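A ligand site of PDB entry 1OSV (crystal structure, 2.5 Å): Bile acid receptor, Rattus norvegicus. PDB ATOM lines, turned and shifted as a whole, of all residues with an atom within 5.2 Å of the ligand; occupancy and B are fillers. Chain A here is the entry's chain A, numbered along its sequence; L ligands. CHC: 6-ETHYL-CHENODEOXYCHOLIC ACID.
The side-chain hydroxyl (OG) of Ser 90 sits at hydrogen-bond distance from the backbone carbonyl oxygen (O) of Met 86, at 2.4 Å. OH of Tyr 127 sits close to OG of Ser 90.
The side-chain hydroxyl (OH) of Tyr 119 is in hydrogen-bond range of an oxygen (O3) of the ligand, 3.1 Å away. An oxygen (O7) of the ligand lies within hydrogen-bond range of the side-chain hydroxyl (OG) of Ser 90 (3.3 Å). An oxygen (O3) of the ligand sits at hydrogen-bond distance from a ring nitrogen (ND1) of His 205 (2.6 Å). The guanidinium group of Arg 89 is in salt-bridge range of an oxygen (OT2) of the ligand (2.9 Å). An oxygen (O7) of the ligand is in hydrogen-bond range of the side-chain hydroxyl (OH) of Tyr 127, 2.9 Å away.
Residues that only touch the ligand: Met 23, Met 48, Ala 49, His 52, Met 86, Phe 87, Phe 94, Ile 110, Met 123, Trp 212 and Trp 227. Hydrophobic or aromatic side chains that line the ligand: Met 23, Met 48, Ala 49, His 52, Met 86, Phe 87, Phe 94, Ile 110, Met 123, Tyr 127, His 205, Trp 212 and Trp 227. Within 4 Å of the ligand: Met 23, Met 48, Ala 49, His 52, Met 86, Phe 87, Arg 89, Ser 90, Phe 94, Ile 110, Tyr 119, Met 123, Tyr 127, His 205, Trp 212 and Trp 227.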
ATOM      1  N   MET A  23     -23.334 -29.713   1.348  1.00  0.00           N
ATOM      2  CA  MET A  23     -23.664 -29.646  -0.085  1.00  0.00           C
ATOM      3  C   MET A  23     -23.447 -30.948  -0.839  1.00  0.00           C
ATOM      4  O   MET A  23     -22.414 -31.611  -0.671  1.00  0.00           O
ATOM      5  CB  MET A  23     -22.841 -28.549  -0.757  1.00  0.00           C
ATOM      6  CG  MET A  23     -23.416 -27.142  -0.635  1.00  0.00           C
ATOM      7  SD  MET A  23     -24.476 -26.708  -2.025  1.00  0.00           S
ATOM      8  CE  MET A  23     -23.227 -26.444  -3.281  1.00  0.00           C
ATOM      9  N   LEU A  45     -23.531 -21.494  -9.747  1.00  0.00           N
ATOM     10  CA  LEU A  45     -23.630 -20.608  -8.593  1.00  0.00           C
ATOM     11  C   LEU A  45     -25.059 -20.527  -8.086  1.00  0.00           C
ATOM     12  O   LEU A  45     -25.296 -20.574  -6.876  1.00  0.00           O
ATOM     13  CB  LEU A  45     -23.158 -19.203  -8.976  1.00  0.00           C
ATOM     14  CG  LEU A  45     -21.702 -18.824  -8.694  1.00  0.00           C
ATOM     15  CD1 LEU A  45     -20.826 -20.062  -8.578  1.00  0.00           C
ATOM     16  CD2 LEU A  45     -21.213 -17.905  -9.791  1.00  0.00           C
ATOM     17  N   MET A  48     -26.127 -23.950  -6.481  1.00  0.00           N
ATOM     18  CA  MET A  48     -25.615 -24.130  -5.126  1.00  0.00           C
ATOM     19  C   MET A  48     -26.455 -23.312  -4.163  1.00  0.00           C
ATOM     20  O   MET A  48     -26.954 -23.838  -3.164  1.00  0.00           O
ATOM     21  CB  MET A  48     -24.170 -23.663  -5.045  1.00  0.00           C
ATOM     22  CG  MET A  48     -23.256 -24.262  -6.066  1.00  0.00           C
ATOM     23  SD  MET A  48     -21.576 -23.675  -5.816  1.00  0.00           S
ATOM     24  CE  MET A  48     -20.650 -25.137  -6.091  1.00  0.00           C
ATOM     25  N   ALA A  49     -26.593 -22.022  -4.451  1.00  0.00           N
ATOM     26  CA  ALA A  49     -27.352 -21.149  -3.581  1.00  0.00           C
ATOM     27  C   ALA A  49     -28.713 -21.760  -3.286  1.00  0.00           C
ATOM     28  O   ALA A  49     -29.197 -21.668  -2.164  1.00  0.00           O
ATOM     29  CB  ALA A  49     -27.517 -19.776  -4.227  1.00  0.00           C
ATOM     30  N   HIS A  52     -27.847 -24.449  -0.750  1.00  0.00           N
ATOM     31  CA  HIS A  52     -27.593 -23.793   0.520  1.00  0.00           C
ATOM     32  C   HIS A  52     -28.887 -23.463   1.256  1.00  0.00           C
ATOM     33  O   HIS A  52     -29.030 -23.777   2.432  1.00  0.00           O
ATOM     34  CB  HIS A  52     -26.783 -22.516   0.293  1.00  0.00           C
ATOM     35  CG  HIS A  52     -26.435 -21.783   1.556  1.00  0.00           C
ATOM     36  ND1 HIS A  52     -27.338 -21.000   2.225  1.00  0.00           N
ATOM     37  CD2 HIS A  52     -25.287 -21.732   2.266  1.00  0.00           C
ATOM     38  CE1 HIS A  52     -26.759 -20.500   3.304  1.00  0.00           C
ATOM     39  NE2 HIS A  52     -25.519 -20.929   3.350  1.00  0.00           N
ATOM     40  N   MET A  86     -26.334 -16.745   4.035  1.00  0.00           N
ATOM     41  CA  MET A  86     -25.522 -17.063   2.869  1.00  0.00           C
ATOM     42  C   MET A  86     -24.238 -16.258   2.916  1.00  0.00           C
ATOM     43  O   MET A  86     -23.168 -16.781   2.607  1.00  0.00           O
ATOM     44  CB  MET A  86     -26.340 -16.769   1.596  1.00  0.00           C
ATOM     45  CG  MET A  86     -25.613 -17.002   0.273  1.00  0.00           C
ATOM     46  SD  MET A  86     -24.652 -15.568  -0.222  1.00  0.00           S
ATOM     47  CE  MET A  86     -25.979 -14.410  -0.572  1.00  0.00           C
ATOM     48  N   PHE A  87     -24.334 -14.993   3.321  1.00  0.00           N
ATOM     49  CA  PHE A  87     -23.127 -14.169   3.424  1.00  0.00           C
ATOM     50  C   PHE A  87     -22.133 -14.763   4.410  1.00  0.00           C
ATOM     51  O   PHE A  87     -20.929 -14.815   4.129  1.00  0.00           O
ATOM     52  CB  PHE A  87     -23.454 -12.736   3.834  1.00  0.00           C
ATOM     53  CG  PHE A  87     -24.082 -11.913   2.741  1.00  0.00           C
ATOM     54  CD1 PHE A  87     -25.180 -11.096   2.991  1.00  0.00           C
ATOM     55  CD2 PHE A  87     -23.581 -11.965   1.437  1.00  0.00           C
ATOM     56  CE1 PHE A  87     -25.785 -10.359   1.966  1.00  0.00           C
ATOM     57  CE2 PHE A  87     -24.170 -11.238   0.401  1.00  0.00           C
ATOM     58  CZ  PHE A  87     -25.267 -10.435   0.664  1.00  0.00           C
ATOM     59  N   ARG A  89     -21.740 -17.915   5.316  1.00  0.00           N
ATOM     60  CA  ARG A  89     -21.151 -19.098   4.693  1.00  0.00           C
ATOM     61  C   ARG A  89     -20.111 -18.663   3.671  1.00  0.00           C
ATOM     62  O   ARG A  89     -19.011 -19.222   3.606  1.00  0.00           O
ATOM     63  CB  ARG A  89     -22.208 -19.939   3.991  1.00  0.00           C
ATOM     64  CG  ARG A  89     -22.675 -21.186   4.733  1.00  0.00           C
ATOM     65  CD  ARG A  89     -22.035 -22.459   4.172  1.00  0.00           C
ATOM     66  NE  ARG A  89     -20.662 -22.668   4.640  1.00  0.00           N
ATOM     67  CZ  ARG A  89     -19.963 -23.785   4.448  1.00  0.00           C
ATOM     68  NH1 ARG A  89     -18.729 -23.884   4.911  1.00  0.00           N
ATOM     69  NH2 ARG A  89     -20.500 -24.818   3.792  1.00  0.00           N
ATOM     70  N   SER A  90     -20.473 -17.673   2.844  1.00  0.00           N
ATOM     71  CA  SER A  90     -19.568 -17.158   1.813  1.00  0.00           C
ATOM     72  C   SER A  90     -18.273 -16.717   2.521  1.00  0.00           C
ATOM     73  O   SER A  90     -17.164 -16.997   2.076  1.00  0.00           O
ATOM     74  CB  SER A  90     -20.188 -15.949   1.110  1.00  0.00           C
ATOM     75  OG  SER A  90     -21.585 -16.127   0.902  1.00  0.00           O
ATOM     76  N   ILE A  93     -16.415 -19.882   3.839  1.00  0.00           N
ATOM     77  CA  ILE A  93     -15.787 -20.551   2.708  1.00  0.00           C
ATOM     78  C   ILE A  93     -14.532 -19.849   2.203  1.00  0.00           C
ATOM     79  O   ILE A  93     -13.462 -20.453   2.134  1.00  0.00           O
ATOM     80  CB  ILE A  93     -16.755 -20.700   1.501  1.00  0.00           C
ATOM     81  CG1 ILE A  93     -17.736 -21.847   1.746  1.00  0.00           C
ATOM     82  CG2 ILE A  93     -15.970 -20.959   0.221  1.00  0.00           C
ATOM     83  CD1 ILE A  93     -17.095 -23.219   1.707  1.00  0.00           C
ATOM     84  N   PHE A  94     -14.662 -18.573   1.869  1.00  0.00           N
ATOM     85  CA  PHE A  94     -13.536 -17.818   1.309  1.00  0.00           C
ATOM     86  C   PHE A  94     -12.281 -17.676   2.148  1.00  0.00           C
ATOM     87  O   PHE A  94     -11.238 -18.207   1.772  1.00  0.00           O
ATOM     88  CB  PHE A  94     -14.045 -16.464   0.810  1.00  0.00           C
ATOM     89  CG  PHE A  94     -14.925 -16.585  -0.400  1.00  0.00           C
ATOM     90  CD1 PHE A  94     -16.122 -15.888  -0.493  1.00  0.00           C
ATOM     91  CD2 PHE A  94     -14.569 -17.461  -1.436  1.00  0.00           C
ATOM     92  CE1 PHE A  94     -16.967 -16.062  -1.599  1.00  0.00           C
ATOM     93  CE2 PHE A  94     -15.391 -17.632  -2.539  1.00  0.00           C
ATOM     94  CZ  PHE A  94     -16.598 -16.942  -2.623  1.00  0.00           C
ATOM     95  N   LEU A 106     -13.907 -21.425  -7.173  1.00  0.00           N
ATOM     96  CA  LEU A 106     -15.277 -20.929  -7.062  1.00  0.00           C
ATOM     97  C   LEU A 106     -15.248 -19.421  -7.232  1.00  0.00           C
ATOM     98  O   LEU A 106     -16.175 -18.832  -7.791  1.00  0.00           O
ATOM     99  CB  LEU A 106     -15.870 -21.281  -5.695  1.00  0.00           C
ATOM    100  CG  LEU A 106     -17.186 -20.565  -5.369  1.00  0.00           C
ATOM    101  CD1 LEU A 106     -18.231 -20.908  -6.414  1.00  0.00           C
ATOM    102  CD2 LEU A 106     -17.672 -20.971  -3.994  1.00  0.00           C
ATOM    103  N   ILE A 110     -17.360 -16.902  -9.870  1.00  0.00           N
ATOM    104  CA  ILE A 110     -18.073 -15.722  -9.380  1.00  0.00           C
ATOM    105  C   ILE A 110     -17.638 -14.502 -10.197  1.00  0.00           C
ATOM    106  O   ILE A 110     -18.458 -13.659 -10.564  1.00  0.00           O
ATOM    107  CB  ILE A 110     -17.793 -15.480  -7.884  1.00  0.00           C
ATOM    108  CG1 ILE A 110     -18.299 -16.673  -7.079  1.00  0.00           C
ATOM    109  CG2 ILE A 110     -18.479 -14.202  -7.436  1.00  0.00           C
ATOM    110  CD1 ILE A 110     -18.130 -16.534  -5.588  1.00  0.00           C
ATOM    111  N   TYR A 119     -19.545  -4.838  -7.653  1.00  0.00           N
ATOM    112  CA  TYR A 119     -20.262  -5.453  -6.548  1.00  0.00           C
ATOM    113  C   TYR A 119     -19.360  -6.479  -5.878  1.00  0.00           C
ATOM    114  O   TYR A 119     -19.264  -6.541  -4.655  1.00  0.00           O
ATOM    115  CB  TYR A 119     -21.533  -6.150  -7.062  1.00  0.00           C
ATOM    116  CG  TYR A 119     -22.365  -6.802  -5.978  1.00  0.00           C
ATOM    117  CD1 TYR A 119     -23.587  -6.241  -5.589  1.00  0.00           C
ATOM    118  CD2 TYR A 119     -21.942  -7.974  -5.345  1.00  0.00           C
ATOM    119  CE1 TYR A 119     -24.370  -6.848  -4.592  1.00  0.00           C
ATOM    120  CE2 TYR A 119     -22.718  -8.589  -4.357  1.00  0.00           C
ATOM    121  CZ  TYR A 119     -23.934  -8.021  -3.991  1.00  0.00           C
ATOM    122  OH  TYR A 119     -24.710  -8.614  -3.023  1.00  0.00           O
ATOM    123  N   ILE A 120     -18.681  -7.290  -6.689  1.00  0.00           N
ATOM    124  CA  ILE A 120     -17.802  -8.321  -6.160  1.00  0.00           C
ATOM    125  C   ILE A 120     -16.633  -7.739  -5.378  1.00  0.00           C
ATOM    126  O   ILE A 120     -16.144  -8.359  -4.442  1.00  0.00           O
ATOM    127  CB  ILE A 120     -17.231  -9.217  -7.287  1.00  0.00           C
ATOM    128  CG1 ILE A 120     -16.171  -8.464  -8.087  1.00  0.00           C
ATOM    129  CG2 ILE A 120     -18.348  -9.644  -8.229  1.00  0.00           C
ATOM    130  CD1 ILE A 120     -15.567  -9.264  -9.230  1.00  0.00           C
ATOM    131  N   MET A 123     -17.880  -6.654  -1.773  1.00  0.00           N
ATOM    132  CA  MET A 123     -18.351  -7.902  -1.182  1.00  0.00           C
ATOM    133  C   MET A 123     -17.136  -8.701  -0.709  1.00  0.00           C
ATOM    134  O   MET A 123     -17.021  -9.030   0.468  1.00  0.00           O
ATOM    135  CB  MET A 123     -19.128  -8.685  -2.239  1.00  0.00           C
ATOM    136  CG  MET A 123     -20.153  -9.650  -1.680  1.00  0.00           C
ATOM    137  SD  MET A 123     -21.424  -8.831  -0.696  1.00  0.00           S
ATOM    138  CE  MET A 123     -21.019  -9.499   0.944  1.00  0.00           C
ATOM    139  N   PHE A 124     -16.221  -8.996  -1.628  1.00  0.00           N
ATOM    140  CA  PHE A 124     -15.019  -9.745  -1.293  1.00  0.00           C
ATOM    141  C   PHE A 124     -14.133  -8.970  -0.341  1.00  0.00           C
ATOM    142  O   PHE A 124     -13.215  -9.521   0.245  1.00  0.00           O
ATOM    143  CB  PHE A 124     -14.208 -10.089  -2.534  1.00  0.00           C
ATOM    144  CG  PHE A 124     -14.706 -11.290  -3.262  1.00  0.00           C
ATOM    145  CD1 PHE A 124     -15.436 -11.165  -4.443  1.00  0.00           C
ATOM    146  CD2 PHE A 124     -14.464 -12.578  -2.750  1.00  0.00           C
ATOM    147  CE1 PHE A 124     -15.919 -12.307  -5.104  1.00  0.00           C
ATOM    148  CE2 PHE A 124     -14.947 -13.727  -3.405  1.00  0.00           C
ATOM    149  CZ  PHE A 124     -15.675 -13.588  -4.585  1.00  0.00           C
ATOM    150  N   TYR A 127     -15.746 -10.055   3.066  1.00  0.00           N
ATOM    151  CA  TYR A 127     -15.309 -11.399   3.430  1.00  0.00           C
ATOM    152  C   TYR A 127     -13.861 -11.385   3.934  1.00  0.00           C
ATOM    153  O   TYR A 127     -13.512 -12.097   4.864  1.00  0.00           O
ATOM    154  CB  TYR A 127     -15.441 -12.336   2.213  1.00  0.00           C
ATOM    155  CG  TYR A 127     -16.857 -12.469   1.664  1.00  0.00           C
ATOM    156  CD1 TYR A 127     -17.069 -12.719   0.291  1.00  0.00           C
ATOM    157  CD2 TYR A 127     -17.968 -12.367   2.495  1.00  0.00           C
ATOM    158  CE1 TYR A 127     -18.371 -12.851  -0.218  1.00  0.00           C
ATOM    159  CE2 TYR A 127     -19.261 -12.508   1.990  1.00  0.00           C
ATOM    160  CZ  TYR A 127     -19.448 -12.756   0.634  1.00  0.00           C
ATOM    161  OH  TYR A 127     -20.735 -12.877   0.137  1.00  0.00           O
ATOM    162  N   HIS A 205     -27.609  -6.496  -2.261  1.00  0.00           N
ATOM    163  CA  HIS A 205     -27.888  -7.789  -2.877  1.00  0.00           C
ATOM    164  C   HIS A 205     -29.238  -7.755  -3.573  1.00  0.00           C
ATOM    165  O   HIS A 205     -29.366  -8.223  -4.698  1.00  0.00           O
ATOM    166  CB  HIS A 205     -27.872  -8.887  -1.808  1.00  0.00           C
ATOM    167  CG  HIS A 205     -28.467 -10.190  -2.254  1.00  0.00           C
ATOM    168  ND1 HIS A 205     -27.695 -11.254  -2.662  1.00  0.00           N
ATOM    169  CD2 HIS A 205     -29.748 -10.599  -2.338  1.00  0.00           C
ATOM    170  CE1 HIS A 205     -28.473 -12.265  -2.980  1.00  0.00           C
ATOM    171  NE2 HIS A 205     -29.732 -11.892  -2.801  1.00  0.00           N
ATOM    172  N   MET A 208     -28.677  -5.587  -6.764  1.00  0.00           N
ATOM    173  CA  MET A 208     -27.824  -6.168  -7.792  1.00  0.00           C
ATOM    174  C   MET A 208     -28.580  -7.216  -8.576  1.00  0.00           C
ATOM    175  O   MET A 208     -28.289  -7.466  -9.747  1.00  0.00           O
ATOM    176  CB  MET A 208     -26.577  -6.784  -7.175  1.00  0.00           C
ATOM    177  CG  MET A 208     -26.773  -8.185  -6.634  1.00  0.00           C
ATOM    178  SD  MET A 208     -26.848  -9.423  -7.936  1.00  0.00           S
ATOM    179  CE  MET A 208     -25.129  -9.812  -8.094  1.00  0.00           C
ATOM    180  N   TRP A 212     -29.357  -8.443 -12.743  1.00  0.00           N
ATOM    181  CA  TRP A 212     -28.271  -9.382 -12.963  1.00  0.00           C
ATOM    182  C   TRP A 212     -28.537 -10.122 -14.222  1.00  0.00           C
ATOM    183  O   TRP A 212     -29.231 -11.146 -14.212  1.00  0.00           O
ATOM    184  CB  TRP A 212     -28.026 -10.201 -11.727  1.00  0.00           C
ATOM    185  CG  TRP A 212     -27.055 -11.333 -11.813  1.00  0.00           C
ATOM    186  CD1 TRP A 212     -26.212 -11.706 -12.802  1.00  0.00           C
ATOM    187  CD2 TRP A 212     -26.863 -12.288 -10.758  1.00  0.00           C
ATOM    188  NE1 TRP A 212     -25.501 -12.839 -12.439  1.00  0.00           N
ATOM    189  CE2 TRP A 212     -25.905 -13.211 -11.181  1.00  0.00           C
ATOM    190  CE3 TRP A 212     -27.425 -12.440  -9.485  1.00  0.00           C
ATOM    191  CZ2 TRP A 212     -25.508 -14.306 -10.399  1.00  0.00           C
ATOM    192  CZ3 TRP A 212     -27.029 -13.506  -8.686  1.00  0.00           C
ATOM    193  CH2 TRP A 212     -26.074 -14.435  -9.160  1.00  0.00           C
ATOM    194  N   TRP A 227     -35.136 -14.905  -2.532  1.00  0.00           N
ATOM    195  CA  TRP A 227     -34.370 -13.716  -2.887  1.00  0.00           C
ATOM    196  C   TRP A 227     -35.334 -12.657  -3.396  1.00  0.00           C
ATOM    197  O   TRP A 227     -34.929 -11.562  -3.809  1.00  0.00           O
ATOM    198  CB  TRP A 227     -33.320 -14.072  -3.941  1.00  0.00           C
ATOM    199  CG  TRP A 227     -32.146 -14.790  -3.345  1.00  0.00           C
ATOM    200  CD1 TRP A 227     -32.031 -15.224  -2.045  1.00  0.00           C
ATOM    201  CD2 TRP A 227     -30.901 -15.115  -3.982  1.00  0.00           C
ATOM    202  NE1 TRP A 227     -30.798 -15.786  -1.848  1.00  0.00           N
ATOM    203  CE2 TRP A 227     -30.081 -15.729  -3.010  1.00  0.00           C
ATOM    204  CE3 TRP A 227     -30.394 -14.946  -5.278  1.00  0.00           C
ATOM    205  CZ2 TRP A 227     -28.775 -16.179  -3.292  1.00  0.00           C
ATOM    206  CZ3 TRP A 227     -29.100 -15.400  -5.565  1.00  0.00           C
ATOM    207  CH2 TRP A 227     -28.302 -16.004  -4.566  1.00  0.00           C
HETATM  208  C1  CHC L   1     -24.823 -14.412  -5.469  1.00  0.00           C
HETATM  209  C2  CHC L   1     -25.460 -13.673  -4.245  1.00  0.00           C
HETATM  210  C3  CHC L   1     -24.591 -12.370  -3.917  1.00  0.00           C
HETATM  211  O3  CHC L   1     -25.149 -11.689  -2.851  1.00  0.00           O
HETATM  212  C4  CHC L   1     -23.067 -12.758  -3.568  1.00  0.00           C
HETATM  213  C5  CHC L   1     -22.382 -13.569  -4.801  1.00  0.00           C
HETATM  214  C6  CHC L   1     -20.868 -14.038  -4.528  1.00  0.00           C
HETATM  215  C7  CHC L   1     -20.779 -15.193  -3.422  1.00  0.00           C
HETATM  216  O7  CHC L   1     -21.157 -14.690  -2.082  1.00  0.00           O
HETATM  217  C8  CHC L   1     -21.663 -16.443  -3.764  1.00  0.00           C
HETATM  218  C9  CHC L   1     -23.227 -16.018  -3.949  1.00  0.00           C
HETATM  219  C10 CHC L   1     -23.321 -14.894  -5.195  1.00  0.00           C
HETATM  220  C11 CHC L   1     -24.058 -17.287  -4.225  1.00  0.00           C
HETATM  221  C12 CHC L   1     -23.982 -18.384  -3.082  1.00  0.00           C
HETATM  222  C13 CHC L   1     -22.489 -18.861  -2.893  1.00  0.00           C
HETATM  223  C14 CHC L   1     -21.617 -17.577  -2.632  1.00  0.00           C
HETATM  224  C15 CHC L   1     -20.200 -18.206  -2.263  1.00  0.00           C
HETATM  225  C16 CHC L   1     -20.629 -19.205  -1.213  1.00  0.00           C
HETATM  226  C17 CHC L   1     -22.128 -19.677  -1.523  1.00  0.00           C
HETATM  227  C18 CHC L   1     -22.037 -19.641  -4.261  1.00  0.00           C
HETATM  228  C19 CHC L   1     -22.951 -15.488  -6.547  1.00  0.00           C
HETATM  229  C20 CHC L   1     -22.291 -21.276  -1.599  1.00  0.00           C
HETATM  230  C21 CHC L   1     -23.851 -21.623  -1.900  1.00  0.00           C
HETATM  231  C22 CHC L   1     -21.898 -21.980  -0.300  1.00  0.00           C
HETATM  232  C23 CHC L   1     -22.059 -23.549  -0.389  1.00  0.00           C
HETATM  233  C24 CHC L   1     -21.701 -24.372   0.793  1.00  0.00           C
HETATM  234  C25 CHC L   1     -19.896 -11.592  -4.697  1.00  0.00           C
HETATM  235  C26 CHC L   1     -20.091 -12.900  -3.946  1.00  0.00           C
HETATM  236  OT1 CHC L   1     -20.619 -24.973   0.773  1.00  0.00           O
HETATM  237  OT2 CHC L   1     -22.508 -24.435   1.755  1.00  0.00           O
